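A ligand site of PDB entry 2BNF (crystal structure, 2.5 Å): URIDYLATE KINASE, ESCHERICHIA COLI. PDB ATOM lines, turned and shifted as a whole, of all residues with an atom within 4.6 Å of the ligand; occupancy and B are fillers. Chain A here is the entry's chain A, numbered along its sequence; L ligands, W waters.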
ATOM      1  N   LYS A  15      -2.216 -37.783 -15.408  1.00  0.00           N
ATOM      2  CA  LYS A  15      -2.154 -36.391 -15.812  1.00  0.00           C
ATOM      3  C   LYS A  15      -1.758 -35.585 -14.586  1.00  0.00           C
ATOM      4  O   LYS A  15      -2.513 -35.527 -13.606  1.00  0.00           O
ATOM      5  CB  LYS A  15      -3.504 -35.917 -16.350  1.00  0.00           C
ATOM      6  CG  LYS A  15      -3.480 -34.530 -16.993  1.00  0.00           C
ATOM      7  CD  LYS A  15      -3.601 -33.407 -15.976  1.00  0.00           C
ATOM      8  CE  LYS A  15      -3.481 -32.056 -16.662  1.00  0.00           C
ATOM      9  NZ  LYS A  15      -3.781 -30.927 -15.732  1.00  0.00           N
ATOM     10  N   SER A  17      -0.736 -31.914 -13.047  1.00  0.00           N
ATOM     11  CA  SER A  17      -0.872 -30.490 -13.289  1.00  0.00           C
ATOM     12  C   SER A  17       0.527 -29.932 -13.041  1.00  0.00           C
ATOM     13  O   SER A  17       1.266 -30.470 -12.213  1.00  0.00           O
ATOM     14  CB  SER A  17      -1.871 -29.896 -12.301  1.00  0.00           C
ATOM     15  OG  SER A  17      -1.885 -28.488 -12.359  1.00  0.00           O
ATOM     16  N   GLY A  18       0.895 -28.880 -13.758  1.00  0.00           N
ATOM     17  CA  GLY A  18       2.211 -28.288 -13.583  1.00  0.00           C
ATOM     18  C   GLY A  18       2.471 -27.896 -12.149  1.00  0.00           C
ATOM     19  O   GLY A  18       3.610 -27.958 -11.674  1.00  0.00           O
ATOM     20  N   GLU A  19       1.411 -27.502 -11.444  1.00  0.00           N
ATOM     21  CA  GLU A  19       1.526 -27.126 -10.057  1.00  0.00           C
ATOM     22  C   GLU A  19       1.968 -28.298  -9.175  1.00  0.00           C
ATOM     23  O   GLU A  19       2.426 -28.109  -8.055  1.00  0.00           O
ATOM     24  CB  GLU A  19       0.196 -26.595  -9.539  1.00  0.00           C
ATOM     25  CG  GLU A  19       0.043 -25.094  -9.654  1.00  0.00           C
ATOM     26  CD  GLU A  19      -0.989 -24.557  -8.682  1.00  0.00           C
ATOM     27  OE1 GLU A  19      -1.109 -23.310  -8.573  1.00  0.00           O
ATOM     28  OE2 GLU A  19      -1.677 -25.373  -8.016  1.00  0.00           O
ATOM     29  N   GLY A  56       1.425 -30.694 -17.073  1.00  0.00           N
ATOM     30  CA  GLY A  56       1.086 -29.320 -17.439  1.00  0.00           C
ATOM     31  C   GLY A  56       2.222 -28.333 -17.253  1.00  0.00           C
ATOM     32  O   GLY A  56       3.339 -28.728 -16.977  1.00  0.00           O
ATOM     33  N   GLY A  57       1.916 -27.040 -17.390  1.00  0.00           N
ATOM     34  CA  GLY A  57       2.954 -26.021 -17.235  1.00  0.00           C
ATOM     35  C   GLY A  57       2.574 -24.817 -16.385  1.00  0.00           C
ATOM     36  O   GLY A  57       3.262 -23.796 -16.421  1.00  0.00           O
ATOM     37  N   GLY A  58       1.504 -24.939 -15.602  1.00  0.00           N
ATOM     38  CA  GLY A  58       1.071 -23.830 -14.772  1.00  0.00           C
ATOM     39  C   GLY A  58       2.038 -23.318 -13.714  1.00  0.00           C
ATOM     40  O   GLY A  58       1.796 -22.271 -13.121  1.00  0.00           O
ATOM     41  N   PHE A  61       4.091 -21.080 -17.011  1.00  0.00           N
ATOM     42  CA  PHE A  61       3.336 -20.172 -17.887  1.00  0.00           C
ATOM     43  C   PHE A  61       1.954 -20.638 -18.330  1.00  0.00           C
ATOM     44  O   PHE A  61       1.678 -21.837 -18.405  1.00  0.00           O
ATOM     45  CB  PHE A  61       4.151 -19.855 -19.136  1.00  0.00           C
ATOM     46  CG  PHE A  61       5.298 -18.932 -18.901  1.00  0.00           C
ATOM     47  CD1 PHE A  61       6.593 -19.310 -19.252  1.00  0.00           C
ATOM     48  CD2 PHE A  61       5.094 -17.679 -18.336  1.00  0.00           C
ATOM     49  CE1 PHE A  61       7.667 -18.450 -19.039  1.00  0.00           C
ATOM     50  CE2 PHE A  61       6.163 -16.807 -18.120  1.00  0.00           C
ATOM     51  CZ  PHE A  61       7.450 -17.188 -18.474  1.00  0.00           C
ATOM     52  N   ARG A  62       1.104 -19.662 -18.626  1.00  0.00           N
ATOM     53  CA  ARG A  62      -0.252 -19.899 -19.113  1.00  0.00           C
ATOM     54  C   ARG A  62      -0.477 -18.882 -20.222  1.00  0.00           C
ATOM     55  O   ARG A  62      -0.253 -17.696 -20.034  1.00  0.00           O
ATOM     56  CB  ARG A  62      -1.277 -19.683 -17.997  1.00  0.00           C
ATOM     57  CG  ARG A  62      -1.213 -20.709 -16.897  1.00  0.00           C
ATOM     58  CD  ARG A  62      -2.228 -20.388 -15.801  1.00  0.00           C
ATOM     59  NE  ARG A  62      -2.305 -21.445 -14.800  1.00  0.00           N
ATOM     60  CZ  ARG A  62      -2.577 -22.719 -15.083  1.00  0.00           C
ATOM     61  NH1 ARG A  62      -2.635 -23.619 -14.110  1.00  0.00           N
ATOM     62  NH2 ARG A  62      -2.791 -23.085 -16.345  1.00  0.00           N
ATOM     63  N   GLY A  63      -0.920 -19.371 -21.377  1.00  0.00           N
ATOM     64  CA  GLY A  63      -1.150 -18.511 -22.524  1.00  0.00           C
ATOM     65  C   GLY A  63      -2.141 -17.389 -22.324  1.00  0.00           C
ATOM     66  O   GLY A  63      -1.890 -16.241 -22.707  1.00  0.00           O
ATOM     67  N   GLY A  76       1.774 -17.078 -26.521  1.00  0.00           N
ATOM     68  CA  GLY A  76       1.656 -17.367 -25.105  1.00  0.00           C
ATOM     69  C   GLY A  76       1.408 -18.845 -24.898  1.00  0.00           C
ATOM     70  O   GLY A  76       1.929 -19.452 -23.946  1.00  0.00           O
ATOM     71  N   ASP A  77       0.616 -19.428 -25.778  1.00  0.00           N
ATOM     72  CA  ASP A  77       0.299 -20.844 -25.698  1.00  0.00           C
ATOM     73  C   ASP A  77       1.519 -21.693 -26.089  1.00  0.00           C
ATOM     74  O   ASP A  77       1.643 -22.839 -25.639  1.00  0.00           O
ATOM     75  CB  ASP A  77      -0.909 -21.187 -26.586  1.00  0.00           C
ATOM     76  CG  ASP A  77      -2.243 -20.731 -25.973  1.00  0.00           C
ATOM     77  OD1 ASP A  77      -2.333 -20.658 -24.738  1.00  0.00           O
ATOM     78  OD2 ASP A  77      -3.203 -20.457 -26.722  1.00  0.00           O
ATOM     79  N   GLY A  80       3.658 -21.735 -23.060  1.00  0.00           N
ATOM     80  CA  GLY A  80       3.032 -22.610 -22.086  1.00  0.00           C
ATOM     81  C   GLY A  80       3.421 -24.039 -22.418  1.00  0.00           C
ATOM     82  O   GLY A  80       3.955 -24.769 -21.573  1.00  0.00           O
ATOM     83  N   MET A  81       3.188 -24.442 -23.660  1.00  0.00           N
ATOM     84  CA  MET A  81       3.525 -25.784 -24.099  1.00  0.00           C
ATOM     85  C   MET A  81       4.990 -26.076 -23.819  1.00  0.00           C
ATOM     86  O   MET A  81       5.323 -27.106 -23.249  1.00  0.00           O
ATOM     87  CB  MET A  81       3.229 -25.967 -25.602  1.00  0.00           C
ATOM     88  CG  MET A  81       1.751 -26.076 -25.909  1.00  0.00           C
ATOM     89  SD  MET A  81       1.302 -26.570 -27.718  1.00  0.00           S
ATOM     90  CE  MET A  81       1.013 -24.806 -28.451  1.00  0.00           C
ATOM     91  N   THR A  84       5.764 -27.188 -20.420  1.00  0.00           N
ATOM     92  CA  THR A  84       5.360 -28.556 -20.103  1.00  0.00           C
ATOM     93  C   THR A  84       6.472 -29.498 -20.545  1.00  0.00           C
ATOM     94  O   THR A  84       6.555 -30.642 -20.105  1.00  0.00           O
ATOM     95  CB  THR A  84       4.060 -28.977 -20.843  1.00  0.00           C
ATOM     96  OG1 THR A  84       4.358 -29.218 -22.219  1.00  0.00           O
ATOM     97  CG2 THR A  84       3.012 -27.887 -20.757  1.00  0.00           C
ATOM     98  N   ALA A 136       4.047 -30.944 -24.305  1.00  0.00           N
ATOM     99  CA  ALA A 136       3.520 -30.015 -25.290  1.00  0.00           C
ATOM    100  C   ALA A 136       2.054 -30.237 -25.598  1.00  0.00           C
ATOM    101  O   ALA A 136       1.573 -29.905 -26.694  1.00  0.00           O
ATOM    102  CB  ALA A 136       4.361 -30.082 -26.564  1.00  0.00           C
ATOM    103  N   GLY A 137       1.349 -30.823 -24.644  1.00  0.00           N
ATOM    104  CA  GLY A 137      -0.080 -31.081 -24.791  1.00  0.00           C
ATOM    105  C   GLY A 137      -0.529 -31.652 -26.120  1.00  0.00           C
ATOM    106  O   GLY A 137      -0.077 -32.709 -26.532  1.00  0.00           O
ATOM    107  N   THR A 138      -1.431 -30.942 -26.785  1.00  0.00           N
ATOM    108  CA  THR A 138      -1.944 -31.402 -28.066  1.00  0.00           C
ATOM    109  C   THR A 138      -1.154 -30.817 -29.232  1.00  0.00           C
ATOM    110  O   THR A 138      -1.381 -31.180 -30.379  1.00  0.00           O
ATOM    111  CB  THR A 138      -3.392 -30.965 -28.245  1.00  0.00           C
ATOM    112  OG1 THR A 138      -3.433 -29.556 -28.490  1.00  0.00           O
ATOM    113  CG2 THR A 138      -4.202 -31.295 -27.000  1.00  0.00           C
ATOM    114  N   GLY A 139      -0.240 -29.914 -28.930  1.00  0.00           N
ATOM    115  CA  GLY A 139       0.557 -29.289 -29.977  1.00  0.00           C
ATOM    116  C   GLY A 139      -0.096 -28.012 -30.492  1.00  0.00           C
ATOM    117  O   GLY A 139       0.525 -27.243 -31.234  1.00  0.00           O
ATOM    118  N   ASN A 140      -1.336 -27.755 -30.103  1.00  0.00           N
ATOM    119  CA  ASN A 140      -2.025 -26.570 -30.570  1.00  0.00           C
ATOM    120  C   ASN A 140      -2.457 -25.619 -29.480  1.00  0.00           C
ATOM    121  O   ASN A 140      -2.778 -26.027 -28.364  1.00  0.00           O
ATOM    122  CB  ASN A 140      -3.289 -26.950 -31.347  1.00  0.00           C
ATOM    123  CG  ASN A 140      -2.971 -27.714 -32.599  1.00  0.00           C
ATOM    124  OD1 ASN A 140      -2.105 -27.310 -33.368  1.00  0.00           O
ATOM    125  ND2 ASN A 140      -3.675 -28.810 -32.832  1.00  0.00           N
ATOM    126  N   PRO A 141      -2.489 -24.319 -29.805  1.00  0.00           N
ATOM    127  CA  PRO A 141      -2.908 -23.310 -28.821  1.00  0.00           C
ATOM    128  C   PRO A 141      -4.414 -23.425 -28.660  1.00  0.00           C
ATOM    129  O   PRO A 141      -5.091 -24.106 -29.444  1.00  0.00           O
ATOM    130  CB  PRO A 141      -2.511 -22.005 -29.495  1.00  0.00           C
ATOM    131  CG  PRO A 141      -2.705 -22.324 -30.953  1.00  0.00           C
ATOM    132  CD  PRO A 141      -2.079 -23.684 -31.066  1.00  0.00           C
ATOM    133  N   PHE A 142      -4.947 -22.740 -27.647  1.00  0.00           N
ATOM    134  CA  PHE A 142      -6.376 -22.743 -27.373  1.00  0.00           C
ATOM    135  C   PHE A 142      -6.802 -24.091 -26.818  1.00  0.00           C
ATOM    136  O   PHE A 142      -7.950 -24.503 -26.963  1.00  0.00           O
ATOM    137  CB  PHE A 142      -7.169 -22.416 -28.636  1.00  0.00           C
ATOM    138  CG  PHE A 142      -6.864 -21.052 -29.179  1.00  0.00           C
ATOM    139  CD1 PHE A 142      -7.114 -19.913 -28.411  1.00  0.00           C
ATOM    140  CD2 PHE A 142      -6.308 -20.901 -30.439  1.00  0.00           C
ATOM    141  CE1 PHE A 142      -6.791 -18.651 -28.895  1.00  0.00           C
ATOM    142  CE2 PHE A 142      -5.985 -19.630 -30.927  1.00  0.00           C
ATOM    143  CZ  PHE A 142      -6.223 -18.516 -30.142  1.00  0.00           C
ATOM    144  N   PHE A 143      -5.859 -24.773 -26.194  1.00  0.00           N
ATOM    145  CA  PHE A 143      -6.107 -26.067 -25.592  1.00  0.00           C
ATOM    146  C   PHE A 143      -5.326 -26.149 -24.291  1.00  0.00           C
ATOM    147  O   PHE A 143      -4.355 -25.416 -24.087  1.00  0.00           O
ATOM    148  CB  PHE A 143      -5.663 -27.201 -26.515  1.00  0.00           C
ATOM    149  CG  PHE A 143      -6.622 -27.481 -27.630  1.00  0.00           C
ATOM    150  CD1 PHE A 143      -6.667 -26.669 -28.753  1.00  0.00           C
ATOM    151  CD2 PHE A 143      -7.520 -28.530 -27.522  1.00  0.00           C
ATOM    152  CE1 PHE A 143      -7.594 -26.893 -29.766  1.00  0.00           C
ATOM    153  CE2 PHE A 143      -8.459 -28.761 -28.526  1.00  0.00           C
ATOM    154  CZ  PHE A 143      -8.497 -27.938 -29.650  1.00  0.00           C
ATOM    155  N   THR A 144      -5.748 -27.037 -23.423  1.00  0.00           N
ATOM    156  CA  THR A 144      -5.103 -27.232 -22.142  1.00  0.00           C
ATOM    157  C   THR A 144      -4.508 -28.635 -22.116  1.00  0.00           C
ATOM    158  O   THR A 144      -4.848 -29.470 -22.953  1.00  0.00           O
ATOM    159  CB  THR A 144      -6.124 -27.121 -21.011  1.00  0.00           C
ATOM    160  OG1 THR A 144      -7.168 -28.088 -21.218  1.00  0.00           O
ATOM    161  CG2 THR A 144      -6.722 -25.730 -20.996  1.00  0.00           C
ATOM    162  N   THR A 145      -3.621 -28.892 -21.168  1.00  0.00           N
ATOM    163  CA  THR A 145      -3.043 -30.209 -21.082  1.00  0.00           C
ATOM    164  C   THR A 145      -4.105 -31.217 -20.651  1.00  0.00           C
ATOM    165  O   THR A 145      -3.944 -32.407 -20.875  1.00  0.00           O
ATOM    166  CB  THR A 145      -1.828 -30.228 -20.130  1.00  0.00           C
ATOM    167  OG1 THR A 145      -2.140 -29.508 -18.940  1.00  0.00           O
ATOM    168  CG2 THR A 145      -0.620 -29.588 -20.813  1.00  0.00           C
ATOM    169  N   ASP A 146      -5.206 -30.761 -20.059  1.00  0.00           N
ATOM    170  CA  ASP A 146      -6.291 -31.682 -19.694  1.00  0.00           C
ATOM    171  C   ASP A 146      -6.798 -32.345 -20.974  1.00  0.00           C
ATOM    172  O   ASP A 146      -6.970 -33.555 -21.024  1.00  0.00           O
ATOM    173  CB  ASP A 146      -7.472 -30.947 -19.031  1.00  0.00           C
ATOM    174  CG  ASP A 146      -7.293 -30.761 -17.544  1.00  0.00           C
ATOM    175  OD1 ASP A 146      -6.416 -31.427 -16.962  1.00  0.00           O
ATOM    176  OD2 ASP A 146      -8.046 -29.960 -16.939  1.00  0.00           O
ATOM    177  N   LYS A 163      -6.513 -38.168 -12.837  1.00  0.00           N
ATOM    178  CA  LYS A 163      -6.268 -36.742 -12.714  1.00  0.00           C
ATOM    179  C   LYS A 163      -5.767 -36.369 -11.338  1.00  0.00           C
ATOM    180  O   LYS A 163      -6.540 -36.327 -10.384  1.00  0.00           O
ATOM    181  CB  LYS A 163      -7.550 -35.958 -13.017  1.00  0.00           C
ATOM    182  CG  LYS A 163      -7.267 -34.491 -13.275  1.00  0.00           C
ATOM    183  CD  LYS A 163      -8.506 -33.632 -13.207  1.00  0.00           C
ATOM    184  CE  LYS A 163      -8.169 -32.210 -13.624  1.00  0.00           C
ATOM    185  NZ  LYS A 163      -6.932 -31.708 -12.956  1.00  0.00           N
HETATM  186  P1  LIG L   1      -1.855 -26.385 -18.699  1.00  0.00           P
HETATM  187  O1  LIG L   1      -3.155 -26.974 -19.088  1.00  0.00           O
HETATM  188  O2  LIG L   1      -0.562 -27.027 -19.098  1.00  0.00           O
HETATM  189  O3  LIG L   1      -1.807 -26.133 -17.104  1.00  0.00           O
HETATM  190  O4  LIG L   1      -1.793 -24.881 -19.106  1.00  0.00           O
HETATM  191  P2  LIG L   1      -1.648 -27.092 -15.873  1.00  0.00           P
HETATM  192  O5  LIG L   1      -0.455 -26.903 -15.081  1.00  0.00           O
HETATM  193  O6  LIG L   1      -1.952 -28.405 -16.353  1.00  0.00           O
HETATM  194  O7  LIG L   1      -2.860 -26.511 -15.044  1.00  0.00           O
HETATM  195  P3  LIG L   1      -4.268 -27.109 -14.675  1.00  0.00           P
HETATM  196  O8  LIG L   1      -5.145 -26.991 -15.933  1.00  0.00           O
HETATM  197  O9  LIG L   1      -3.951 -28.535 -14.296  1.00  0.00           O
HETATM  198  O10 LIG L   1      -4.852 -26.324 -13.527  1.00  0.00           O
HETATM  199  C1  LIG L   1      -0.528 -24.276 -19.347  1.00  0.00           C
HETATM  200  C2  LIG L   1      -0.535 -23.614 -20.675  1.00  0.00           C
HETATM  201  O11 LIG L   1      -0.044 -24.529 -21.688  1.00  0.00           O
HETATM  202  C3  LIG L   1      -0.586 -24.136 -22.957  1.00  0.00           C
HETATM  203  C4  LIG L   1      -1.565 -22.986 -22.640  1.00  0.00           C
HETATM  204  O12 LIG L   1      -0.951 -21.740 -22.860  1.00  0.00           O
HETATM  205  C5  LIG L   1      -1.892 -23.229 -21.186  1.00  0.00           C
HETATM  206  O13 LIG L   1      -2.357 -22.077 -20.505  1.00  0.00           O
HETATM  207  N1  LIG L   1      -1.177 -25.296 -23.677  1.00  0.00           N
HETATM  208  C6  LIG L   1      -1.289 -26.557 -23.079  1.00  0.00           C
HETATM  209  C7  LIG L   1      -1.542 -25.113 -25.033  1.00  0.00           C
HETATM  210  O14 LIG L   1      -1.754 -24.023 -25.530  1.00  0.00           O
HETATM  211  N2  LIG L   1      -1.865 -26.284 -25.714  1.00  0.00           N
HETATM  212  C8  LIG L   1      -2.050 -27.559 -25.174  1.00  0.00           C
HETATM  213  O15 LIG L   1      -2.638 -28.422 -25.848  1.00  0.00           O
HETATM  214  C9  LIG L   1      -1.697 -27.667 -23.760  1.00  0.00           C
HETATM  215  O   HOH W   1      -3.871 -20.356 -22.006  1.00  0.00           O
HETATM  216  O   HOH W   2      -4.533 -31.293 -12.751  1.00  0.00           O
HETATM  217  O   HOH W   3      -4.859 -28.622 -18.099  1.00  0.00           O
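N of Gly 58 sits at hydrogen-bond distance from O5 of the ligand (2.8 Å). NH1 of Arg 62 is in salt-bridge range of O10 of the ligand, at 3.5 Å. An oxygen (O1) of the ligand sits at hydrogen-bond distance from the side-chain hydroxyl (OG1) of Thr 145 (2.7 Å). The backbone NH (N) of Gly 57 sits at hydrogen-bond distance from an oxygen (O2) of the ligand (3.0 Å). An oxygen (O9) of the ligand is in salt-bridge range of the side-chain amino group (NZ) of Lys 15 (2.8 Å). The side-chain hydroxyl (OG) of Ser 17 sits at hydrogen-bond distance from an oxygen (O9) of the ligand, 2.8 Å away. The backbone carbonyl oxygen (O) of Phe 143 sits close to a nitrogen (N2) of the ligand, 3.1 Å away. The side-chain carboxylate (OD1) of Asp 77 sits at hydrogen-bond distance from an oxygen (O12) of the ligand. The side-chain sulfur (SD) of Met 81 sits close to a nitrogen (N2) of the ligand (3.8 Å). N of Thr 138 lies within hydrogen-bond range of O15 of the ligand, 2.9 Å away. The backbone NH (N) of Gly 63 sits at hydrogen-bond distance from an oxygen (O12) of the ligand. The backbone NH (N) of Thr 145 lies within hydrogen-bond range of an oxygen (O1) of the ligand (2.9 Å). OG1 of Thr 138 is in hydrogen-bond range of O15 of the ligand, 3.0 Å away. The backbone NH (N) of Gly 18 is in hydrogen-bond range of an oxygen (O5) of the ligand. O of Asn 140 sits at hydrogen-bond distance from N2 of the ligand, at 2.8 Å.
O of Met 81 lies within hydrogen-bond range of OG1 of Thr 84 (2.5 Å). NZ of Lys 15 lies within salt-bridge range of OD1 of Asp 146. The backbone NH (N) of Asn 140 lies within hydrogen-bond range of the side-chain sulfur (SD) of Met 81 (3.7 Å). N of Phe 142 lies within hydrogen-bond range of OD2 of Asp 77 (3.0 Å). N of Asn 140 sits close to OG1 of Thr 138.
Gly 56 touches the ligand (CA to O2, 3.3 Å). Phe 61 touches the ligand. O of Gly 76 touches O12 of the ligand (3.8 Å). Gly 80 touches the ligand (C to O11, 3.6 Å). CA of Gly 137 touches O15 of the ligand (3.8 Å). Pro 141 touches the ligand (CA to O14, 3.6 Å). Thr 144 touches the ligand (C to C9, 3.4 Å). Hydrophobic or aromatic side chains that line the ligand: Met 81 and Phe 143. The nearest printed residue that does not touch the ligand is Thr 84 (4.03 Å).
Water W3 lies within hydrogen-bond range of an oxygen (O1) of the ligand, the backbone NH (N) of Asp 146, the side-chain hydroxyl (OG1) of Thr 145 and the side-chain amino group (NZ) of Lys 15. Water W1 lies within hydrogen-bond range of O13 of the ligand (2.7 Å), OD1 of Asp 77 (3.1 Å) and N of Gly 63 (3.2 Å). Water W2 lies within hydrogen-bond range of the side-chain amino group (NZ) of Lys 163 (2.4 Å), the side-chain amino group (NZ) of Lys 15 (3.1 Å) and an oxygen (O9) of the ligand (3.2 Å).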
